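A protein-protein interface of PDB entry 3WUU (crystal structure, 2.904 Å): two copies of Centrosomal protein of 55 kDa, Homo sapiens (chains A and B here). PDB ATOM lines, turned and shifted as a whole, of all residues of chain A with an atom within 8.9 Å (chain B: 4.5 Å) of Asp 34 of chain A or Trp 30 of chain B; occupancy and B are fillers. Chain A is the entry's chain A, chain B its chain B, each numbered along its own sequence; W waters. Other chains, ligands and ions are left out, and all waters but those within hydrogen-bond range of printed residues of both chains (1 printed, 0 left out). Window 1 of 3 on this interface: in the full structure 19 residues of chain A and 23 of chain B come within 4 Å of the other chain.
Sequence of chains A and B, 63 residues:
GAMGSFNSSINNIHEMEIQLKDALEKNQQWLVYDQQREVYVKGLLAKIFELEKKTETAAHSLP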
ATOM      1  N   ALA A  23       9.418   6.337  27.257  1.00  0.00           N
ATOM      2  CA  ALA A  23       8.276   7.222  27.073  1.00  0.00           C
ATOM      3  C   ALA A  23       8.728   8.659  26.814  1.00  0.00           C
ATOM      4  O   ALA A  23       8.079   9.395  26.073  1.00  0.00           O
ATOM      5  CB  ALA A  23       7.349   7.158  28.274  1.00  0.00           C
ATOM      6  N   LEU A  24       9.845   9.052  27.421  1.00  0.00           N
ATOM      7  CA  LEU A  24      10.354  10.410  27.265  1.00  0.00           C
ATOM      8  C   LEU A  24      10.828  10.676  25.848  1.00  0.00           C
ATOM      9  O   LEU A  24      10.601  11.754  25.304  1.00  0.00           O
ATOM     10  CB  LEU A  24      11.489  10.697  28.252  1.00  0.00           C
ATOM     11  CG  LEU A  24      11.090  11.152  29.657  1.00  0.00           C
ATOM     12  CD1 LEU A  24      12.330  11.477  30.472  1.00  0.00           C
ATOM     13  CD2 LEU A  24      10.143  12.341  29.596  1.00  0.00           C
ATOM     14  N   LYS A  26       9.757   9.192  23.284  1.00  0.00           N
ATOM     15  CA  LYS A  26       8.644   8.939  22.372  1.00  0.00           C
ATOM     16  C   LYS A  26       7.707  10.130  22.250  1.00  0.00           C
ATOM     17  O   LYS A  26       7.225  10.439  21.160  1.00  0.00           O
ATOM     18  CB  LYS A  26       7.868   7.688  22.789  1.00  0.00           C
ATOM     19  CG  LYS A  26       8.525   6.393  22.374  1.00  0.00           C
ATOM     20  CD  LYS A  26       7.724   5.183  22.817  1.00  0.00           C
ATOM     21  CE  LYS A  26       8.428   3.893  22.414  1.00  0.00           C
ATOM     22  NZ  LYS A  26       7.771   2.667  22.952  1.00  0.00           N
ATOM     23  N   ASN A  27       7.436  10.784  23.375  1.00  0.00           N
ATOM     24  CA  ASN A  27       6.715  12.048  23.352  1.00  0.00           C
ATOM     25  C   ASN A  27       7.572  13.062  22.613  1.00  0.00           C
ATOM     26  O   ASN A  27       7.075  13.998  21.988  1.00  0.00           O
ATOM     27  CB  ASN A  27       6.415  12.525  24.773  1.00  0.00           C
ATOM     28  CG  ASN A  27       5.591  11.522  25.556  1.00  0.00           C
ATOM     29  OD1 ASN A  27       5.039  10.581  24.983  1.00  0.00           O
ATOM     30  ND2 ASN A  27       5.495  11.719  26.867  1.00  0.00           N
ATOM     31  N   GLN A  28       8.879  12.840  22.672  1.00  0.00           N
ATOM     32  CA  GLN A  28       9.846  13.690  22.001  1.00  0.00           C
ATOM     33  C   GLN A  28       9.858  13.424  20.495  1.00  0.00           C
ATOM     34  O   GLN A  28      10.179  14.312  19.707  1.00  0.00           O
ATOM     35  CB  GLN A  28      11.235  13.473  22.609  1.00  0.00           C
ATOM     36  CG  GLN A  28      12.262  14.529  22.238  1.00  0.00           C
ATOM     37  CD  GLN A  28      11.864  15.933  22.674  1.00  0.00           C
ATOM     38  OE1 GLN A  28      11.107  16.116  23.628  1.00  0.00           O
ATOM     39  NE2 GLN A  28      12.381  16.933  21.970  1.00  0.00           N
ATOM     40  N   GLN A  29       9.500  12.203  20.102  1.00  0.00           N
ATOM     41  CA  GLN A  29       9.389  11.852  18.686  1.00  0.00           C
ATOM     42  C   GLN A  29       8.032  12.261  18.111  1.00  0.00           C
ATOM     43  O   GLN A  29       7.920  12.579  16.928  1.00  0.00           O
ATOM     44  CB  GLN A  29       9.641  10.357  18.473  1.00  0.00           C
ATOM     45  CG  GLN A  29      11.109   9.974  18.546  1.00  0.00           C
ATOM     46  CD  GLN A  29      11.331   8.475  18.571  1.00  0.00           C
ATOM     47  OE1 GLN A  29      10.385   7.694  18.536  1.00  0.00           O
ATOM     48  NE2 GLN A  29      12.591   8.067  18.633  1.00  0.00           N
ATOM     49  N   TRP A  30       7.005  12.257  18.953  1.00  0.00           N
ATOM     50  CA  TRP A  30       5.693  12.745  18.553  1.00  0.00           C
ATOM     51  C   TRP A  30       5.758  14.211  18.133  1.00  0.00           C
ATOM     52  O   TRP A  30       4.975  14.662  17.298  1.00  0.00           O
ATOM     53  CB  TRP A  30       4.682  12.576  19.688  1.00  0.00           C
ATOM     54  CG  TRP A  30       4.048  11.230  19.726  1.00  0.00           C
ATOM     55  CD1 TRP A  30       4.257  10.249  20.649  1.00  0.00           C
ATOM     56  CD2 TRP A  30       3.103  10.707  18.789  1.00  0.00           C
ATOM     57  NE1 TRP A  30       3.497   9.147  20.346  1.00  0.00           N
ATOM     58  CE2 TRP A  30       2.780   9.403  19.208  1.00  0.00           C
ATOM     59  CE3 TRP A  30       2.499  11.216  17.633  1.00  0.00           C
ATOM     60  CZ2 TRP A  30       1.878   8.600  18.513  1.00  0.00           C
ATOM     61  CZ3 TRP A  30       1.605  10.419  16.945  1.00  0.00           C
ATOM     62  CH2 TRP A  30       1.301   9.124  17.388  1.00  0.00           C
ATOM     63  N   LEU A  31       6.693  14.951  18.720  1.00  0.00           N
ATOM     64  CA  LEU A  31       6.855  16.365  18.406  1.00  0.00           C
ATOM     65  C   LEU A  31       7.307  16.542  16.964  1.00  0.00           C
ATOM     66  O   LEU A  31       6.729  17.325  16.213  1.00  0.00           O
ATOM     67  CB  LEU A  31       7.861  17.019  19.358  1.00  0.00           C
ATOM     68  CG  LEU A  31       8.122  18.510  19.133  1.00  0.00           C
ATOM     69  CD1 LEU A  31       6.830  19.296  19.265  1.00  0.00           C
ATOM     70  CD2 LEU A  31       9.175  19.035  20.099  1.00  0.00           C
ATOM     71  N   VAL A  32       8.344  15.804  16.585  1.00  0.00           N
ATOM     72  CA  VAL A  32       8.884  15.878  15.236  1.00  0.00           C
ATOM     73  C   VAL A  32       7.850  15.416  14.215  1.00  0.00           C
ATOM     74  O   VAL A  32       7.684  16.035  13.164  1.00  0.00           O
ATOM     75  CB  VAL A  32      10.168  15.038  15.110  1.00  0.00           C
ATOM     76  CG1 VAL A  32      10.643  14.990  13.666  1.00  0.00           C
ATOM     77  CG2 VAL A  32      11.248  15.601  16.014  1.00  0.00           C
ATOM     78  N   TYR A  33       7.144  14.339  14.539  1.00  0.00           N
ATOM     79  CA  TYR A  33       6.114  13.811  13.656  1.00  0.00           C
ATOM     80  C   TYR A  33       4.990  14.817  13.444  1.00  0.00           C
ATOM     81  O   TYR A  33       4.588  15.088  12.313  1.00  0.00           O
ATOM     82  CB  TYR A  33       5.547  12.504  14.211  1.00  0.00           C
ATOM     83  CG  TYR A  33       4.417  11.933  13.384  1.00  0.00           C
ATOM     84  CD1 TYR A  33       4.663  11.337  12.152  1.00  0.00           C
ATOM     85  CD2 TYR A  33       3.106  11.987  13.835  1.00  0.00           C
ATOM     86  CE1 TYR A  33       3.634  10.814  11.394  1.00  0.00           C
ATOM     87  CE2 TYR A  33       2.069  11.467  13.084  1.00  0.00           C
ATOM     88  CZ  TYR A  33       2.339  10.881  11.866  1.00  0.00           C
ATOM     89  OH  TYR A  33       1.308  10.363  11.116  1.00  0.00           O
ATOM     90  N   ASP A  34       4.488  15.374  14.540  1.00  0.00           N
ATOM     91  CA  ASP A  34       3.385  16.320  14.467  1.00  0.00           C
ATOM     92  C   ASP A  34       3.788  17.643  13.820  1.00  0.00           C
ATOM     93  O   ASP A  34       2.966  18.304  13.184  1.00  0.00           O
ATOM     94  CB  ASP A  34       2.798  16.571  15.852  1.00  0.00           C
ATOM     95  CG  ASP A  34       1.485  17.307  15.791  1.00  0.00           C
ATOM     96  OD1 ASP A  34       0.497  16.697  15.335  1.00  0.00           O
ATOM     97  OD2 ASP A  34       1.438  18.489  16.192  1.00  0.00           O
ATOM     98  N   GLN A  35       5.048  18.030  13.985  1.00  0.00           N
ATOM     99  CA  GLN A  35       5.557  19.247  13.362  1.00  0.00           C
ATOM    100  C   GLN A  35       5.569  19.098  11.848  1.00  0.00           C
ATOM    101  O   GLN A  35       5.426  20.078  11.116  1.00  0.00           O
ATOM    102  CB  GLN A  35       6.961  19.572  13.867  1.00  0.00           C
ATOM    103  CG  GLN A  35       6.989  20.281  15.203  1.00  0.00           C
ATOM    104  CD  GLN A  35       8.399  20.561  15.677  1.00  0.00           C
ATOM    105  OE1 GLN A  35       9.320  19.787  15.413  1.00  0.00           O
ATOM    106  NE2 GLN A  35       8.579  21.676  16.375  1.00  0.00           N
ATOM    107  N   GLN A  36       5.746  17.861  11.393  1.00  0.00           N
ATOM    108  CA  GLN A  36       5.742  17.551   9.971  1.00  0.00           C
ATOM    109  C   GLN A  36       4.320  17.499   9.420  1.00  0.00           C
ATOM    110  O   GLN A  36       4.063  17.952   8.301  1.00  0.00           O
ATOM    111  CB  GLN A  36       6.456  16.223   9.709  1.00  0.00           C
ATOM    112  CG  GLN A  36       7.968  16.294   9.821  1.00  0.00           C
ATOM    113  CD  GLN A  36       8.589  17.222   8.794  1.00  0.00           C
ATOM    114  OE1 GLN A  36       8.497  16.988   7.587  1.00  0.00           O
ATOM    115  NE2 GLN A  36       9.223  18.289   9.269  1.00  0.00           N
ATOM    116  N   ARG A  37       3.399  16.939  10.200  1.00  0.00           N
ATOM    117  CA  ARG A  37       2.004  16.888   9.785  1.00  0.00           C
ATOM    118  C   ARG A  37       1.460  18.301   9.625  1.00  0.00           C
ATOM    119  O   ARG A  37       0.648  18.567   8.737  1.00  0.00           O
ATOM    120  CB  ARG A  37       1.154  16.088  10.777  1.00  0.00           C
ATOM    121  CG  ARG A  37      -0.347  16.123  10.479  1.00  0.00           C
ATOM    122  CD  ARG A  37      -1.094  15.018  11.206  1.00  0.00           C
ATOM    123  NE  ARG A  37      -0.754  14.971  12.622  1.00  0.00           N
ATOM    124  CZ  ARG A  37      -0.854  13.882  13.378  1.00  0.00           C
ATOM    125  NH1 ARG A  37      -1.283  12.745  12.849  1.00  0.00           N
ATOM    126  NH2 ARG A  37      -0.522  13.928  14.661  1.00  0.00           N
ATOM    127  N   GLU A  38       1.927  19.209  10.477  1.00  0.00           N
ATOM    128  CA  GLU A  38       1.502  20.603  10.408  1.00  0.00           C
ATOM    129  C   GLU A  38       1.967  21.272   9.120  1.00  0.00           C
ATOM    130  O   GLU A  38       1.269  22.127   8.575  1.00  0.00           O
ATOM    131  CB  GLU A  38       1.988  21.385  11.629  1.00  0.00           C
ATOM    132  CG  GLU A  38       1.165  21.119  12.877  1.00  0.00           C
ATOM    133  CD  GLU A  38      -0.308  21.421  12.668  1.00  0.00           C
ATOM    134  OE1 GLU A  38      -0.619  22.490  12.098  1.00  0.00           O
ATOM    135  OE2 GLU A  38      -1.153  20.589  13.064  1.00  0.00           O
ATOM    136  N   VAL A  39       3.143  20.881   8.637  1.00  0.00           N
ATOM    137  CA  VAL A  39       3.629  21.366   7.354  1.00  0.00           C
ATOM    138  C   VAL A  39       2.649  20.952   6.266  1.00  0.00           C
ATOM    139  O   VAL A  39       2.255  21.762   5.429  1.00  0.00           O
ATOM    140  CB  VAL A  39       5.036  20.818   7.027  1.00  0.00           C
ATOM    141  CG1 VAL A  39       5.390  21.075   5.568  1.00  0.00           C
ATOM    142  CG2 VAL A  39       6.077  21.437   7.944  1.00  0.00           C
ATOM    143  N   TYR A  40       2.240  19.688   6.308  1.00  0.00           N
ATOM    144  CA  TYR A  40       1.307  19.139   5.331  1.00  0.00           C
ATOM    145  C   TYR A  40      -0.062  19.811   5.418  1.00  0.00           C
ATOM    146  O   TYR A  40      -0.649  20.173   4.400  1.00  0.00           O
ATOM    147  CB  TYR A  40       1.169  17.629   5.533  1.00  0.00           C
ATOM    148  CG  TYR A  40       0.363  16.929   4.464  1.00  0.00           C
ATOM    149  CD1 TYR A  40       0.858  16.792   3.173  1.00  0.00           C
ATOM    150  CD2 TYR A  40      -0.884  16.390   4.750  1.00  0.00           C
ATOM    151  CE1 TYR A  40       0.128  16.146   2.191  1.00  0.00           C
ATOM    152  CE2 TYR A  40      -1.621  15.741   3.776  1.00  0.00           C
ATOM    153  CZ  TYR A  40      -1.113  15.623   2.497  1.00  0.00           C
ATOM    154  OH  TYR A  40      -1.847  14.976   1.526  1.00  0.00           O
ATOM    155  N   VAL A  41      -0.561  19.978   6.639  1.00  0.00           N
ATOM    156  CA  VAL A  41      -1.857  20.609   6.861  1.00  0.00           C
ATOM    157  C   VAL A  41      -1.885  22.047   6.343  1.00  0.00           C
ATOM    158  O   VAL A  41      -2.817  22.443   5.636  1.00  0.00           O
ATOM    159  CB  VAL A  41      -2.248  20.580   8.346  1.00  0.00           C
ATOM    160  CG1 VAL A  41      -3.468  21.453   8.593  1.00  0.00           C
ATOM    161  CG2 VAL A  41      -2.516  19.150   8.785  1.00  0.00           C
ATOM    162  N   LYS A  42      -0.860  22.820   6.685  1.00  0.00           N
ATOM    163  CA  LYS A  42      -0.754  24.190   6.202  1.00  0.00           C
ATOM    164  C   LYS A  42      -0.712  24.233   4.676  1.00  0.00           C
ATOM    165  O   LYS A  42      -1.201  25.182   4.061  1.00  0.00           O
ATOM    166  CB  LYS A  42       0.473  24.884   6.798  1.00  0.00           C
ATOM    167  CG  LYS A  42       0.344  25.225   8.281  1.00  0.00           C
ATOM    168  CD  LYS A  42       1.582  25.960   8.777  1.00  0.00           C
ATOM    169  CE  LYS A  42       1.495  26.296  10.261  1.00  0.00           C
ATOM    170  NZ  LYS A  42       1.665  25.101  11.135  1.00  0.00           N
ATOM    171  N   LYS B  26       0.833  11.914  29.007  1.00  0.00           N
ATOM    172  CA  LYS B  26       1.032  12.730  27.818  1.00  0.00           C
ATOM    173  C   LYS B  26       1.155  11.884  26.558  1.00  0.00           C
ATOM    174  O   LYS B  26       0.714  12.290  25.482  1.00  0.00           O
ATOM    175  CB  LYS B  26       2.253  13.626  27.984  1.00  0.00           C
ATOM    176  CG  LYS B  26       2.061  14.714  29.008  1.00  0.00           C
ATOM    177  CD  LYS B  26       3.083  15.810  28.826  1.00  0.00           C
ATOM    178  CE  LYS B  26       2.801  16.978  29.748  1.00  0.00           C
ATOM    179  NZ  LYS B  26       3.361  16.740  31.099  1.00  0.00           N
ATOM    180  N   ASN B  27       1.754  10.709  26.694  1.00  0.00           N
ATOM    181  CA  ASN B  27       1.866   9.788  25.571  1.00  0.00           C
ATOM    182  C   ASN B  27       0.494   9.336  25.084  1.00  0.00           C
ATOM    183  O   ASN B  27       0.288   9.136  23.884  1.00  0.00           O
ATOM    184  CB  ASN B  27       2.707   8.574  25.952  1.00  0.00           C
ATOM    185  CG  ASN B  27       3.034   7.708  24.766  1.00  0.00           C
ATOM    186  OD1 ASN B  27       2.408   6.671  24.546  1.00  0.00           O
ATOM    187  ND2 ASN B  27       4.007   8.140  23.975  1.00  0.00           N
ATOM    188  N   GLN B  28      -0.434   9.177  26.028  1.00  0.00           N
ATOM    189  CA  GLN B  28      -1.817   8.833  25.718  1.00  0.00           C
ATOM    190  C   GLN B  28      -2.504   9.997  25.028  1.00  0.00           C
ATOM    191  O   GLN B  28      -3.270   9.815  24.083  1.00  0.00           O
ATOM    192  CB  GLN B  28      -2.590   8.483  26.999  1.00  0.00           C
ATOM    193  CG  GLN B  28      -2.650   7.006  27.367  1.00  0.00           C
ATOM    194  CD  GLN B  28      -3.723   6.691  28.401  1.00  0.00           C
ATOM    195  OE1 GLN B  28      -4.880   7.085  28.252  1.00  0.00           O
ATOM    196  NE2 GLN B  28      -3.338   5.984  29.460  1.00  0.00           N
ATOM    197  N   GLN B  29      -2.238  11.196  25.527  1.00  0.00           N
ATOM    198  CA  GLN B  29      -2.820  12.402  24.956  1.00  0.00           C
ATOM    199  C   GLN B  29      -2.327  12.596  23.527  1.00  0.00           C
ATOM    200  O   GLN B  29      -3.087  13.004  22.656  1.00  0.00           O
ATOM    201  CB  GLN B  29      -2.488  13.623  25.820  1.00  0.00           C
ATOM    202  CG  GLN B  29      -3.137  13.574  27.201  1.00  0.00           C
ATOM    203  CD  GLN B  29      -2.560  14.593  28.175  1.00  0.00           C
ATOM    204  OE1 GLN B  29      -1.404  15.006  28.057  1.00  0.00           O
ATOM    205  NE2 GLN B  29      -3.365  14.994  29.148  1.00  0.00           N
ATOM    206  N   TRP B  30      -1.053  12.287  23.294  1.00  0.00           N
ATOM    207  CA  TRP B  30      -0.481  12.328  21.954  1.00  0.00           C
ATOM    208  C   TRP B  30      -1.196  11.350  21.025  1.00  0.00           C
ATOM    209  O   TRP B  30      -1.436  11.658  19.857  1.00  0.00           O
ATOM    210  CB  TRP B  30       1.008  11.992  21.989  1.00  0.00           C
ATOM    211  CG  TRP B  30       1.919  13.162  22.252  1.00  0.00           C
ATOM    212  CD1 TRP B  30       2.680  13.373  23.366  1.00  0.00           C
ATOM    213  CD2 TRP B  30       2.181  14.267  21.375  1.00  0.00           C
ATOM    214  NE1 TRP B  30       3.395  14.539  23.238  1.00  0.00           N
ATOM    215  CE2 TRP B  30       3.106  15.108  22.025  1.00  0.00           C
ATOM    216  CE3 TRP B  30       1.720  14.629  20.105  1.00  0.00           C
ATOM    217  CZ2 TRP B  30       3.581  16.283  21.449  1.00  0.00           C
ATOM    218  CZ3 TRP B  30       2.192  15.798  19.535  1.00  0.00           C
ATOM    219  CH2 TRP B  30       3.112  16.611  20.207  1.00  0.00           C
ATOM    220  N   LEU B  31      -1.527  10.171  21.546  1.00  0.00           N
ATOM    221  CA  LEU B  31      -2.209   9.147  20.758  1.00  0.00           C
ATOM    222  C   LEU B  31      -3.597   9.589  20.312  1.00  0.00           C
ATOM    223  O   LEU B  31      -3.919   9.552  19.125  1.00  0.00           O
ATOM    224  CB  LEU B  31      -2.316   7.844  21.550  1.00  0.00           C
ATOM    225  CG  LEU B  31      -1.294   6.752  21.238  1.00  0.00           C
ATOM    226  CD1 LEU B  31       0.115   7.309  21.271  1.00  0.00           C
ATOM    227  CD2 LEU B  31      -1.440   5.606  22.224  1.00  0.00           C
ATOM    228  N   VAL B  32      -4.415  10.002  21.272  1.00  0.00           N
ATOM    229  CA  VAL B  32      -5.784  10.416  20.994  1.00  0.00           C
ATOM    230  C   VAL B  32      -5.809  11.651  20.105  1.00  0.00           C
ATOM    231  O   VAL B  32      -6.640  11.767  19.208  1.00  0.00           O
ATOM    232  CB  VAL B  32      -6.545  10.715  22.293  1.00  0.00           C
ATOM    233  CG1 VAL B  32      -7.994  11.035  21.991  1.00  0.00           C
ATOM    234  CG2 VAL B  32      -6.448   9.531  23.242  1.00  0.00           C
ATOM    235  N   TYR B  33      -4.889  12.572  20.368  1.00  0.00           N
ATOM    236  CA  TYR B  33      -4.734  13.775  19.559  1.00  0.00           C
ATOM    237  C   TYR B  33      -4.369  13.398  18.130  1.00  0.00           C
ATOM    238  O   TYR B  33      -4.899  13.968  17.179  1.00  0.00           O
ATOM    239  CB  TYR B  33      -3.663  14.675  20.179  1.00  0.00           C
ATOM    240  CG  TYR B  33      -3.095  15.760  19.290  1.00  0.00           C
ATOM    241  CD1 TYR B  33      -3.781  16.948  19.082  1.00  0.00           C
ATOM    242  CD2 TYR B  33      -1.846  15.613  18.697  1.00  0.00           C
ATOM    243  CE1 TYR B  33      -3.251  17.948  18.287  1.00  0.00           C
ATOM    244  CE2 TYR B  33      -1.311  16.605  17.903  1.00  0.00           C
ATOM    245  CZ  TYR B  33      -2.014  17.771  17.700  1.00  0.00           C
ATOM    246  OH  TYR B  33      -1.475  18.760  16.907  1.00  0.00           O
ATOM    247  N   ASP B  34      -3.478  12.420  17.989  1.00  0.00           N
ATOM    248  CA  ASP B  34      -3.019  11.984  16.676  1.00  0.00           C
ATOM    249  C   ASP B  34      -4.166  11.466  15.824  1.00  0.00           C
ATOM    250  O   ASP B  34      -4.278  11.804  14.645  1.00  0.00           O
ATOM    251  CB  ASP B  34      -1.951  10.899  16.806  1.00  0.00           C
ATOM    252  CG  ASP B  34      -1.490  10.375  15.460  1.00  0.00           C
ATOM    253  OD1 ASP B  34      -0.660  11.048  14.813  1.00  0.00           O
ATOM    254  OD2 ASP B  34      -1.957   9.292  15.048  1.00  0.00           O
HETATM  255  O   HOH W   1      -1.584  21.344  15.552  1.00  0.00           O
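OD1 of Asn 27 of chain A sits at hydrogen-bond distance from ND2 of Asn 27 of chain B (2.8 Å). The side-chain carboxylate (OD2) of Asp 34 of chain A sits at hydrogen-bond distance from the side-chain hydroxyl (OH) of Tyr 33 of chain B. The side-chain carboxylate (OD1) of Asp 34 of chain B lies within salt-bridge range of the guanidinium group (NH1) of Arg 37 of chain A (2.7 Å).
O of Ala 23 of chain A lies close to OD1 of Asn 27 of chain A, 3.4 Å away. The guanidinium group (NH2) of Arg 37 of chain A lies within salt-bridge range of the side-chain carboxylate (OD1) of Asp 34 of chain A (3.0 Å).
Among the printed residues, merely in contact across the chains: Trp 30 of chain A with Asp 34 of chain B (3.2 Å), Tyr 33 of chain A with Asp 34 of chain B (3.3 Å), Trp 30 of chain A with Trp 30 of chain B (3.5 Å), Trp 30 of chain A with Leu 31 of chain B (3.5 Å), Trp 30 of chain A with Asn 27 of chain B (3.8 Å), Asp 34 of chain A with Trp 30 of chain B (3.8 Å), Asn 27 of chain A with Lys 26 of chain B (3.9 Å) and Asn 27 of chain A with Trp 30 of chain B (3.9 Å).
Of the printed residues of chain B, Asn 27 of chain A touches Lys 26 (3.9 Å), Asn 27 (2.8 Å) and Trp 30 (3.9 Å). Of the printed residues of chain B, Trp 30 of chain A touches Asn 27, Trp 30, Leu 31 and Asp 34. Printed residues of chain B within 4 Å of Tyr 33 of chain A: Asp 34 (3.3 Å). Of chain B, only Trp 30 and Tyr 33 come within 4 Å of Asp 34 of chain A. Of chain A, only Asn 27 (3.9 Å), Trp 30 (3.5 Å) and Asp 34 (3.8 Å) come within 4 Å of Trp 30 of chain B. Of the printed residues of chain A, Leu 31 of chain B touches Trp 30. Printed residues of chain A within 4 Å of Asp 34 of chain B: Trp 30 (3.2 Å), Tyr 33 (3.3 Å) and Arg 37 (2.7 Å). The nearest printed residue of chain B that does not touch Asp 34 of chain A is Asp 34 of chain B (5.8 Å). The nearest printed residue of chain A that does not touch Tyr 33 of chain B is Glu 38 of chain A (4.3 Å).
Of the 19 printed residues of chain A, 5 touch a printed residue of chain B. Printed residues of chain B that touch a printed residue of chain A: Lys 26, Asn 27, Trp 30, Leu 31, Tyr 33 and Asp 34. Among the printed residues, 11 pairs touch across the chains.
Asn 27 of chain A touches its own counterpart, Asn 27 of chain B. Trp 30 of chain A touches Leu 31 of chain B, but with the chains exchanged Leu 31 of chain A does not touch Trp 30 of chain B (4.2 Å). Trp 30 of chain A touches Asp 34 of chain B, and with the chains exchanged Asp 34 of chain A touches Trp 30 of chain B. Tyr 33 of chain A touches Asp 34 of chain B, and with the chains exchanged Asp 34 of chain A touches Tyr 33 of chain B. Of the 11 pairs that touch across the chains among the printed residues, 8 have their exchanged pair printed and touching as well.
Water W1 lies within hydrogen-bond range of the side-chain carboxylate of Glu 38 of chain A (2.6 Å) and the side-chain hydroxyl of Tyr 33 of chain B (2.9 Å).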
